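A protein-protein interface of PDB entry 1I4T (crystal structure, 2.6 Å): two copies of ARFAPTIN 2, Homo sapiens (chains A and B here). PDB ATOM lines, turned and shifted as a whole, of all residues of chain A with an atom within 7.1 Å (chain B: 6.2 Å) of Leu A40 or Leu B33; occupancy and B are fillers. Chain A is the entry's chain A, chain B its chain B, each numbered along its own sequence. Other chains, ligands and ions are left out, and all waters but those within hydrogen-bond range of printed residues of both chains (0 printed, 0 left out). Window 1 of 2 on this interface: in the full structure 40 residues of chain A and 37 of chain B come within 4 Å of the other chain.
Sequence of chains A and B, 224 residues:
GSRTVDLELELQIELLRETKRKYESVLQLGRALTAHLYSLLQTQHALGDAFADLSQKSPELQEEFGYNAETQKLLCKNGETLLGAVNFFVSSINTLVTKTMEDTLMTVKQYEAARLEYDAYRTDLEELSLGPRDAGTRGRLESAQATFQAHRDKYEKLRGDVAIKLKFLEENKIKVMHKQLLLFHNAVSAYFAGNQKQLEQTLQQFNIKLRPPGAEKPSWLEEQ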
ATOM      1  N   ALA A  35     -14.695 -34.706  30.585  1.00  0.00           N
ATOM      2  CA  ALA A  35     -13.621 -34.638  29.600  1.00  0.00           C
ATOM      3  C   ALA A  35     -13.176 -33.200  29.427  1.00  0.00           C
ATOM      4  O   ALA A  35     -12.003 -32.857  29.615  1.00  0.00           O
ATOM      5  CB  ALA A  35     -14.091 -35.196  28.264  1.00  0.00           C
ATOM      6  N   HIS A  36     -14.136 -32.366  29.050  1.00  0.00           N
ATOM      7  CA  HIS A  36     -13.903 -30.951  28.835  1.00  0.00           C
ATOM      8  C   HIS A  36     -13.278 -30.275  30.051  1.00  0.00           C
ATOM      9  O   HIS A  36     -12.363 -29.479  29.919  1.00  0.00           O
ATOM     10  CB  HIS A  36     -15.220 -30.307  28.454  1.00  0.00           C
ATOM     11  CG  HIS A  36     -15.833 -30.919  27.240  1.00  0.00           C
ATOM     12  ND1 HIS A  36     -17.184 -30.871  26.974  1.00  0.00           N
ATOM     13  CD2 HIS A  36     -15.269 -31.597  26.212  1.00  0.00           C
ATOM     14  CE1 HIS A  36     -17.427 -31.493  25.835  1.00  0.00           C
ATOM     15  NE2 HIS A  36     -16.282 -31.941  25.351  1.00  0.00           N
ATOM     16  N   LEU A  37     -13.750 -30.617  31.238  1.00  0.00           N
ATOM     17  CA  LEU A  37     -13.200 -30.020  32.443  1.00  0.00           C
ATOM     18  C   LEU A  37     -11.720 -30.391  32.558  1.00  0.00           C
ATOM     19  O   LEU A  37     -10.866 -29.540  32.844  1.00  0.00           O
ATOM     20  CB  LEU A  37     -13.982 -30.504  33.667  1.00  0.00           C
ATOM     21  CG  LEU A  37     -13.988 -29.538  34.843  1.00  0.00           C
ATOM     22  CD1 LEU A  37     -14.153 -28.121  34.320  1.00  0.00           C
ATOM     23  CD2 LEU A  37     -15.107 -29.881  35.802  1.00  0.00           C
ATOM     24  N   TYR A  38     -11.429 -31.662  32.301  1.00  0.00           N
ATOM     25  CA  TYR A  38     -10.067 -32.199  32.353  1.00  0.00           C
ATOM     26  C   TYR A  38      -9.161 -31.519  31.320  1.00  0.00           C
ATOM     27  O   TYR A  38      -8.001 -31.246  31.605  1.00  0.00           O
ATOM     28  CB  TYR A  38     -10.110 -33.718  32.125  1.00  0.00           C
ATOM     29  CG  TYR A  38      -8.766 -34.402  31.999  1.00  0.00           C
ATOM     30  CD1 TYR A  38      -7.923 -34.559  33.102  1.00  0.00           C
ATOM     31  CD2 TYR A  38      -8.347 -34.907  30.775  1.00  0.00           C
ATOM     32  CE1 TYR A  38      -6.702 -35.206  32.981  1.00  0.00           C
ATOM     33  CE2 TYR A  38      -7.136 -35.549  30.641  1.00  0.00           C
ATOM     34  CZ  TYR A  38      -6.311 -35.700  31.739  1.00  0.00           C
ATOM     35  OH  TYR A  38      -5.091 -36.334  31.570  1.00  0.00           O
ATOM     36  N   SER A  39      -9.686 -31.244  30.130  1.00  0.00           N
ATOM     37  CA  SER A  39      -8.899 -30.574  29.101  1.00  0.00           C
ATOM     38  C   SER A  39      -8.621 -29.120  29.524  1.00  0.00           C
ATOM     39  O   SER A  39      -7.520 -28.598  29.332  1.00  0.00           O
ATOM     40  CB  SER A  39      -9.656 -30.535  27.773  1.00  0.00           C
ATOM     41  OG  SER A  39     -10.142 -31.801  27.391  1.00  0.00           O
ATOM     42  N   LEU A  40      -9.640 -28.466  30.080  1.00  0.00           N
ATOM     43  CA  LEU A  40      -9.512 -27.080  30.500  1.00  0.00           C
ATOM     44  C   LEU A  40      -8.446 -26.987  31.581  1.00  0.00           C
ATOM     45  O   LEU A  40      -7.451 -26.282  31.435  1.00  0.00           O
ATOM     46  CB  LEU A  40     -10.854 -26.562  31.036  1.00  0.00           C
ATOM     47  CG  LEU A  40     -10.861 -25.087  31.443  1.00  0.00           C
ATOM     48  CD1 LEU A  40     -10.629 -24.240  30.208  1.00  0.00           C
ATOM     49  CD2 LEU A  40     -12.180 -24.718  32.089  1.00  0.00           C
ATOM     50  N   LEU A  41      -8.673 -27.723  32.661  1.00  0.00           N
ATOM     51  CA  LEU A  41      -7.773 -27.778  33.801  1.00  0.00           C
ATOM     52  C   LEU A  41      -6.292 -27.814  33.394  1.00  0.00           C
ATOM     53  O   LEU A  41      -5.470 -27.051  33.911  1.00  0.00           O
ATOM     54  CB  LEU A  41      -8.099 -29.025  34.617  1.00  0.00           C
ATOM     55  CG  LEU A  41      -8.395 -28.865  36.106  1.00  0.00           C
ATOM     56  CD1 LEU A  41      -9.514 -27.847  36.298  1.00  0.00           C
ATOM     57  CD2 LEU A  41      -8.782 -30.216  36.708  1.00  0.00           C
ATOM     58  N   GLN A  42      -5.965 -28.719  32.475  1.00  0.00           N
ATOM     59  CA  GLN A  42      -4.602 -28.897  32.002  1.00  0.00           C
ATOM     60  C   GLN A  42      -4.039 -27.663  31.338  1.00  0.00           C
ATOM     61  O   GLN A  42      -2.907 -27.260  31.611  1.00  0.00           O
ATOM     62  CB  GLN A  42      -4.539 -30.062  31.020  1.00  0.00           C
ATOM     63  CG  GLN A  42      -4.576 -31.421  31.683  1.00  0.00           C
ATOM     64  CD  GLN A  42      -4.589 -32.539  30.675  1.00  0.00           C
ATOM     65  OE1 GLN A  42      -5.508 -32.648  29.868  1.00  0.00           O
ATOM     66  NE2 GLN A  42      -3.564 -33.376  30.709  1.00  0.00           N
ATOM     67  N   THR A  43      -4.820 -27.083  30.436  1.00  0.00           N
ATOM     68  CA  THR A  43      -4.399 -25.881  29.733  1.00  0.00           C
ATOM     69  C   THR A  43      -4.026 -24.811  30.774  1.00  0.00           C
ATOM     70  O   THR A  43      -2.902 -24.302  30.805  1.00  0.00           O
ATOM     71  CB  THR A  43      -5.539 -25.338  28.840  1.00  0.00           C
ATOM     72  OG1 THR A  43      -5.955 -26.344  27.911  1.00  0.00           O
ATOM     73  CG2 THR A  43      -5.068 -24.134  28.069  1.00  0.00           C
ATOM     74  N   GLN A  44      -4.966 -24.500  31.649  1.00  0.00           N
ATOM     75  CA  GLN A  44      -4.727 -23.492  32.655  1.00  0.00           C
ATOM     76  C   GLN A  44      -3.395 -23.731  33.365  1.00  0.00           C
ATOM     77  O   GLN A  44      -2.747 -22.781  33.825  1.00  0.00           O
ATOM     78  CB  GLN A  44      -5.898 -23.467  33.635  1.00  0.00           C
ATOM     79  CG  GLN A  44      -7.230 -23.335  32.910  1.00  0.00           C
ATOM     80  CD  GLN A  44      -8.410 -23.317  33.847  1.00  0.00           C
ATOM     81  OE1 GLN A  44      -8.491 -24.110  34.790  1.00  0.00           O
ATOM     82  NE2 GLN A  44      -9.342 -22.419  33.588  1.00  0.00           N
ATOM     83  N   HIS A  45      -2.980 -24.993  33.441  1.00  0.00           N
ATOM     84  CA  HIS A  45      -1.714 -25.335  34.080  1.00  0.00           C
ATOM     85  C   HIS A  45      -0.584 -24.905  33.153  1.00  0.00           C
ATOM     86  O   HIS A  45       0.359 -24.241  33.575  1.00  0.00           O
ATOM     87  CB  HIS A  45      -1.618 -26.844  34.330  1.00  0.00           C
ATOM     88  CG  HIS A  45      -0.315 -27.285  34.927  1.00  0.00           C
ATOM     89  ND1 HIS A  45      -0.104 -27.365  36.288  1.00  0.00           N
ATOM     90  CD2 HIS A  45       0.844 -27.680  34.345  1.00  0.00           C
ATOM     91  CE1 HIS A  45       1.127 -27.792  36.518  1.00  0.00           C
ATOM     92  NE2 HIS A  45       1.722 -27.991  35.355  1.00  0.00           N
ATOM     93  N   ALA A  46      -0.687 -25.282  31.884  1.00  0.00           N
ATOM     94  CA  ALA A  46       0.341 -24.932  30.919  1.00  0.00           C
ATOM     95  C   ALA A  46       0.423 -23.410  30.855  1.00  0.00           C
ATOM     96  O   ALA A  46       1.485 -22.813  31.065  1.00  0.00           O
ATOM     97  CB  ALA A  46      -0.009 -25.508  29.551  1.00  0.00           C
ATOM     98  N   LEU A  47      -0.724 -22.807  30.557  1.00  0.00           N
ATOM     99  CA  LEU A  47      -0.891 -21.367  30.471  1.00  0.00           C
ATOM    100  C   LEU A  47      -0.225 -20.740  31.695  1.00  0.00           C
ATOM    101  O   LEU A  47       0.468 -19.737  31.595  1.00  0.00           O
ATOM    102  CB  LEU A  47      -2.385 -21.047  30.459  1.00  0.00           C
ATOM    103  CG  LEU A  47      -2.883 -19.822  29.705  1.00  0.00           C
ATOM    104  CD1 LEU A  47      -2.380 -19.825  28.277  1.00  0.00           C
ATOM    105  CD2 LEU A  47      -4.399 -19.831  29.740  1.00  0.00           C
ATOM    106  N   GLN A  72      -4.243 -18.357  36.689  1.00  0.00           N
ATOM    107  CA  GLN A  72      -4.384 -19.586  35.935  1.00  0.00           C
ATOM    108  C   GLN A  72      -3.963 -20.767  36.824  1.00  0.00           C
ATOM    109  O   GLN A  72      -4.512 -21.866  36.714  1.00  0.00           O
ATOM    110  CB  GLN A  72      -3.522 -19.498  34.679  1.00  0.00           C
ATOM    111  CG  GLN A  72      -4.210 -19.892  33.383  1.00  0.00           C
ATOM    112  CD  GLN A  72      -5.580 -19.256  33.182  1.00  0.00           C
ATOM    113  OE1 GLN A  72      -5.750 -18.044  33.301  1.00  0.00           O
ATOM    114  NE2 GLN A  72      -6.568 -20.085  32.856  1.00  0.00           N
ATOM    115  N   CYS A  76      -6.535 -23.693  38.192  1.00  0.00           N
ATOM    116  CA  CYS A  76      -6.194 -25.080  37.940  1.00  0.00           C
ATOM    117  C   CYS A  76      -6.389 -25.904  39.199  1.00  0.00           C
ATOM    118  O   CYS A  76      -7.004 -26.966  39.164  1.00  0.00           O
ATOM    119  CB  CYS A  76      -4.746 -25.198  37.487  1.00  0.00           C
ATOM    120  SG  CYS A  76      -4.225 -26.891  37.142  1.00  0.00           S
ATOM    121  N   TYR A 191     -16.859 -23.987  43.426  1.00  0.00           N
ATOM    122  CA  TYR A 191     -15.841 -23.691  42.423  1.00  0.00           C
ATOM    123  C   TYR A 191     -15.946 -22.230  41.992  1.00  0.00           C
ATOM    124  O   TYR A 191     -15.696 -21.888  40.828  1.00  0.00           O
ATOM    125  CB  TYR A 191     -16.010 -24.596  41.206  1.00  0.00           C
ATOM    126  CG  TYR A 191     -15.082 -24.275  40.059  1.00  0.00           C
ATOM    127  CD1 TYR A 191     -13.699 -24.317  40.217  1.00  0.00           C
ATOM    128  CD2 TYR A 191     -15.588 -23.943  38.808  1.00  0.00           C
ATOM    129  CE1 TYR A 191     -12.842 -24.039  39.152  1.00  0.00           C
ATOM    130  CE2 TYR A 191     -14.742 -23.663  37.736  1.00  0.00           C
ATOM    131  CZ  TYR A 191     -13.371 -23.712  37.914  1.00  0.00           C
ATOM    132  OH  TYR A 191     -12.537 -23.421  36.856  1.00  0.00           O
ATOM    133  N   GLN B  28      -1.065 -20.940  21.120  1.00  0.00           N
ATOM    134  CA  GLN B  28      -1.560 -22.307  21.021  1.00  0.00           C
ATOM    135  C   GLN B  28      -2.442 -22.582  22.233  1.00  0.00           C
ATOM    136  O   GLN B  28      -3.646 -22.831  22.092  1.00  0.00           O
ATOM    137  CB  GLN B  28      -0.401 -23.306  20.973  1.00  0.00           C
ATOM    138  CG  GLN B  28       0.261 -23.423  19.603  1.00  0.00           C
ATOM    139  CD  GLN B  28      -0.694 -23.917  18.514  1.00  0.00           C
ATOM    140  OE1 GLN B  28      -1.657 -23.231  18.149  1.00  0.00           O
ATOM    141  NE2 GLN B  28      -0.428 -25.115  17.995  1.00  0.00           N
ATOM    142  N   LEU B  29      -1.844 -22.522  23.424  1.00  0.00           N
ATOM    143  CA  LEU B  29      -2.585 -22.748  24.657  1.00  0.00           C
ATOM    144  C   LEU B  29      -3.845 -21.889  24.687  1.00  0.00           C
ATOM    145  O   LEU B  29      -4.781 -22.183  25.422  1.00  0.00           O
ATOM    146  CB  LEU B  29      -1.734 -22.396  25.869  1.00  0.00           C
ATOM    147  CG  LEU B  29      -0.486 -23.197  26.236  1.00  0.00           C
ATOM    148  CD1 LEU B  29       0.016 -22.707  27.604  1.00  0.00           C
ATOM    149  CD2 LEU B  29      -0.820 -24.687  26.308  1.00  0.00           C
ATOM    150  N   GLY B  30      -3.862 -20.825  23.890  1.00  0.00           N
ATOM    151  CA  GLY B  30      -5.013 -19.940  23.854  1.00  0.00           C
ATOM    152  C   GLY B  30      -6.116 -20.468  22.970  1.00  0.00           C
ATOM    153  O   GLY B  30      -7.297 -20.296  23.273  1.00  0.00           O
ATOM    154  N   ARG B  31      -5.741 -21.099  21.863  1.00  0.00           N
ATOM    155  CA  ARG B  31      -6.729 -21.671  20.945  1.00  0.00           C
ATOM    156  C   ARG B  31      -7.375 -22.856  21.652  1.00  0.00           C
ATOM    157  O   ARG B  31      -8.571 -23.106  21.522  1.00  0.00           O
ATOM    158  CB  ARG B  31      -6.056 -22.164  19.668  1.00  0.00           C
ATOM    159  CG  ARG B  31      -5.219 -21.124  18.986  1.00  0.00           C
ATOM    160  CD  ARG B  31      -5.169 -21.351  17.502  1.00  0.00           C
ATOM    161  NE  ARG B  31      -4.660 -20.165  16.829  1.00  0.00           N
ATOM    162  CZ  ARG B  31      -3.395 -19.774  16.878  1.00  0.00           C
ATOM    163  NH1 ARG B  31      -2.508 -20.486  17.564  1.00  0.00           N
ATOM    164  NH2 ARG B  31      -3.027 -18.659  16.259  1.00  0.00           N
ATOM    165  N   ALA B  32      -6.557 -23.579  22.404  1.00  0.00           N
ATOM    166  CA  ALA B  32      -7.036 -24.715  23.145  1.00  0.00           C
ATOM    167  C   ALA B  32      -8.055 -24.216  24.160  1.00  0.00           C
ATOM    168  O   ALA B  32      -9.175 -24.723  24.228  1.00  0.00           O
ATOM    169  CB  ALA B  32      -5.884 -25.391  23.848  1.00  0.00           C
ATOM    170  N   LEU B  33      -7.661 -23.214  24.942  1.00  0.00           N
ATOM    171  CA  LEU B  33      -8.527 -22.650  25.963  1.00  0.00           C
ATOM    172  C   LEU B  33      -9.884 -22.333  25.365  1.00  0.00           C
ATOM    173  O   LEU B  33     -10.924 -22.617  25.962  1.00  0.00           O
ATOM    174  CB  LEU B  33      -7.900 -21.384  26.532  1.00  0.00           C
ATOM    175  CG  LEU B  33      -8.697 -20.670  27.623  1.00  0.00           C
ATOM    176  CD1 LEU B  33      -8.874 -21.559  28.836  1.00  0.00           C
ATOM    177  CD2 LEU B  33      -7.966 -19.417  28.001  1.00  0.00           C
ATOM    178  N   THR B  34      -9.874 -21.746  24.180  1.00  0.00           N
ATOM    179  CA  THR B  34     -11.112 -21.405  23.494  1.00  0.00           C
ATOM    180  C   THR B  34     -11.951 -22.667  23.276  1.00  0.00           C
ATOM    181  O   THR B  34     -13.098 -22.764  23.711  1.00  0.00           O
ATOM    182  CB  THR B  34     -10.810 -20.787  22.117  1.00  0.00           C
ATOM    183  OG1 THR B  34      -9.932 -19.673  22.284  1.00  0.00           O
ATOM    184  CG2 THR B  34     -12.085 -20.309  21.448  1.00  0.00           C
ATOM    185  N   ALA B  35     -11.345 -23.627  22.584  1.00  0.00           N
ATOM    186  CA  ALA B  35     -11.958 -24.909  22.246  1.00  0.00           C
ATOM    187  C   ALA B  35     -12.601 -25.589  23.448  1.00  0.00           C
ATOM    188  O   ALA B  35     -13.813 -25.772  23.515  1.00  0.00           O
ATOM    189  CB  ALA B  35     -10.906 -25.818  21.649  1.00  0.00           C
ATOM    190  N   HIS B  36     -11.768 -25.960  24.402  1.00  0.00           N
ATOM    191  CA  HIS B  36     -12.237 -26.619  25.597  1.00  0.00           C
ATOM    192  C   HIS B  36     -13.321 -25.841  26.323  1.00  0.00           C
ATOM    193  O   HIS B  36     -14.200 -26.429  26.941  1.00  0.00           O
ATOM    194  CB  HIS B  36     -11.042 -26.874  26.507  1.00  0.00           C
ATOM    195  CG  HIS B  36      -9.969 -27.684  25.853  1.00  0.00           C
ATOM    196  ND1 HIS B  36      -8.690 -27.783  26.361  1.00  0.00           N
ATOM    197  CD2 HIS B  36      -9.984 -28.432  24.724  1.00  0.00           C
ATOM    198  CE1 HIS B  36      -7.964 -28.556  25.573  1.00  0.00           C
ATOM    199  NE2 HIS B  36      -8.726 -28.963  24.571  1.00  0.00           N
ATOM    200  N   LEU B  37     -13.269 -24.515  26.232  1.00  0.00           N
ATOM    201  CA  LEU B  37     -14.246 -23.656  26.902  1.00  0.00           C
ATOM    202  C   LEU B  37     -15.573 -23.672  26.164  1.00  0.00           C
ATOM    203  O   LEU B  37     -16.640 -23.671  26.769  1.00  0.00           O
ATOM    204  CB  LEU B  37     -13.689 -22.233  26.988  1.00  0.00           C
ATOM    205  CG  LEU B  37     -14.435 -21.200  27.837  1.00  0.00           C
ATOM    206  CD1 LEU B  37     -14.649 -21.743  29.251  1.00  0.00           C
ATOM    207  CD2 LEU B  37     -13.621 -19.899  27.873  1.00  0.00           C
ATOM    208  N   TYR B  38     -15.503 -23.700  24.845  1.00  0.00           N
ATOM    209  CA  TYR B  38     -16.710 -23.730  24.033  1.00  0.00           C
ATOM    210  C   TYR B  38     -17.474 -25.015  24.345  1.00  0.00           C
ATOM    211  O   TYR B  38     -18.683 -24.994  24.588  1.00  0.00           O
ATOM    212  CB  TYR B  38     -16.340 -23.686  22.549  1.00  0.00           C
ATOM    213  CG  TYR B  38     -17.529 -23.685  21.621  1.00  0.00           C
ATOM    214  CD1 TYR B  38     -18.463 -22.654  21.662  1.00  0.00           C
ATOM    215  CD2 TYR B  38     -17.725 -24.718  20.693  1.00  0.00           C
ATOM    216  CE1 TYR B  38     -19.565 -22.644  20.805  1.00  0.00           C
ATOM    217  CE2 TYR B  38     -18.830 -24.716  19.827  1.00  0.00           C
ATOM    218  CZ  TYR B  38     -19.743 -23.675  19.893  1.00  0.00           C
ATOM    219  OH  TYR B  38     -20.845 -23.657  19.067  1.00  0.00           O
ATOM    220  N   LEU B  40     -17.440 -26.883  26.959  1.00  0.00           N
ATOM    221  CA  LEU B  40     -18.013 -26.807  28.280  1.00  0.00           C
ATOM    222  C   LEU B  40     -19.356 -26.059  28.334  1.00  0.00           C
ATOM    223  O   LEU B  40     -20.210 -26.365  29.167  1.00  0.00           O
ATOM    224  CB  LEU B  40     -17.003 -26.150  29.211  1.00  0.00           C
ATOM    225  CG  LEU B  40     -17.308 -26.241  30.699  1.00  0.00           C
ATOM    226  CD1 LEU B  40     -17.310 -27.688  31.135  1.00  0.00           C
ATOM    227  CD2 LEU B  40     -16.266 -25.467  31.472  1.00  0.00           C
ATOM    228  N   LEU B  83     -16.054 -16.251  27.104  1.00  0.00           N
ATOM    229  CA  LEU B  83     -15.584 -16.777  25.827  1.00  0.00           C
ATOM    230  C   LEU B  83     -15.330 -15.636  24.845  1.00  0.00           C
ATOM    231  O   LEU B  83     -14.402 -15.688  24.040  1.00  0.00           O
ATOM    232  CB  LEU B  83     -16.616 -17.750  25.246  1.00  0.00           C
ATOM    233  CG  LEU B  83     -16.142 -18.452  23.974  1.00  0.00           C
ATOM    234  CD1 LEU B  83     -14.960 -19.339  24.298  1.00  0.00           C
ATOM    235  CD2 LEU B  83     -17.256 -19.273  23.398  1.00  0.00           C
ATOM    236  N   VAL B  86     -11.956 -14.188  25.873  1.00  0.00           N
ATOM    237  CA  VAL B  86     -10.874 -15.093  25.484  1.00  0.00           C
ATOM    238  C   VAL B  86     -10.660 -15.084  23.968  1.00  0.00           C
ATOM    239  O   VAL B  86      -9.529 -15.179  23.496  1.00  0.00           O
ATOM    240  CB  VAL B  86     -11.169 -16.553  25.946  1.00  0.00           C
ATOM    241  CG1 VAL B  86     -10.012 -17.474  25.589  1.00  0.00           C
ATOM    242  CG2 VAL B  86     -11.407 -16.582  27.449  1.00  0.00           C
ATOM    243  N   PHE B 184      -8.043  -9.760  29.647  1.00  0.00           N
ATOM    244  CA  PHE B 184      -8.106 -11.194  29.861  1.00  0.00           C
ATOM    245  C   PHE B 184      -8.305 -11.472  31.337  1.00  0.00           C
ATOM    246  O   PHE B 184      -9.276 -12.113  31.722  1.00  0.00           O
ATOM    247  CB  PHE B 184      -6.808 -11.849  29.392  1.00  0.00           C
ATOM    248  CG  PHE B 184      -6.787 -13.343  29.542  1.00  0.00           C
ATOM    249  CD1 PHE B 184      -7.313 -14.167  28.546  1.00  0.00           C
ATOM    250  CD2 PHE B 184      -6.222 -13.934  30.674  1.00  0.00           C
ATOM    251  CE1 PHE B 184      -7.272 -15.568  28.672  1.00  0.00           C
ATOM    252  CE2 PHE B 184      -6.176 -15.331  30.811  1.00  0.00           C
ATOM    253  CZ  PHE B 184      -6.704 -16.146  29.806  1.00  0.00           C
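The backbone carbonyl oxygen of Ser A39 lies close to a ring nitrogen (ND1) of His B36 (3.3 Å).
ND1 of His B36 sits at hydrogen-bond distance from OG1 of Thr A43 (3.5 Å).
The side-chain hydroxyl (OG) of Ser A39 lies within hydrogen-bond range of the backbone carbonyl oxygen (O) of Ala A35, at 3.1 Å.
The side-chain hydroxyl (OG1) of Thr A43 is in hydrogen-bond range of the backbone carbonyl oxygen (O) of Ser A39, at 3.1 Å.
His A36 touches Leu B40.
Leu A40 touches Leu B33.
Leu A40 touches His B36.
CG2 of Thr A43 touches O of Leu B29, at 3.3 Å.
Ala A46 touches Leu B29 (C to CD1, 3.4 Å).
N of Leu A47 touches CD1 of Leu B29, at 3.0 Å.
Leu A47 touches Leu B33 (CD2 to CD2, 3.99 Å).
Phe B184 touches Gln A72.
His A36 touches Leu B40, and with the chains exchanged Leu A40 touches His B36.
5 positions are printed for both chains.
Of the 10 pairs that touch across the chains among the printed residues, 2 have their exchanged pair printed and touching as well.
Leu A40 touches just these residues of chain B: Leu B33 and His B36.
Printed residues of chain A within 4 Å of Leu B33: Leu A40 (3.5 Å) and Leu A47 (3.99 Å).
No residue of chain A comes within 4 Å of Ala B32.
Printed residues of chain B within 4 Å of Thr A43: Leu B29 and His B36.
Of the printed residues of chain B, Ala A46 touches Leu B29.
Of the printed residues of chain B, Ser A39 touches His B36 (3.2 Å).
Printed residues of chain A within 4 Å of Leu B40: His A36.
Leu B37 touches none of the printed residues of chain A.
The nearest residue of chain B that does not touch Leu A40 is Leu B40 (4.2 Å).
Of the 16 printed residues of chain A, 7 touch a printed residue of chain B.
Hydrophobic or aromatic side chains of chain A that line the printed part of chain B: His A36, Leu A40, Ala A46 and Leu A47.
Hydrophobic or aromatic side chains of chain B that line the printed part of chain A: Leu B29, Leu B33, His B36 and Phe B184.
Among the printed residues, 10 pairs touch across the chains.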
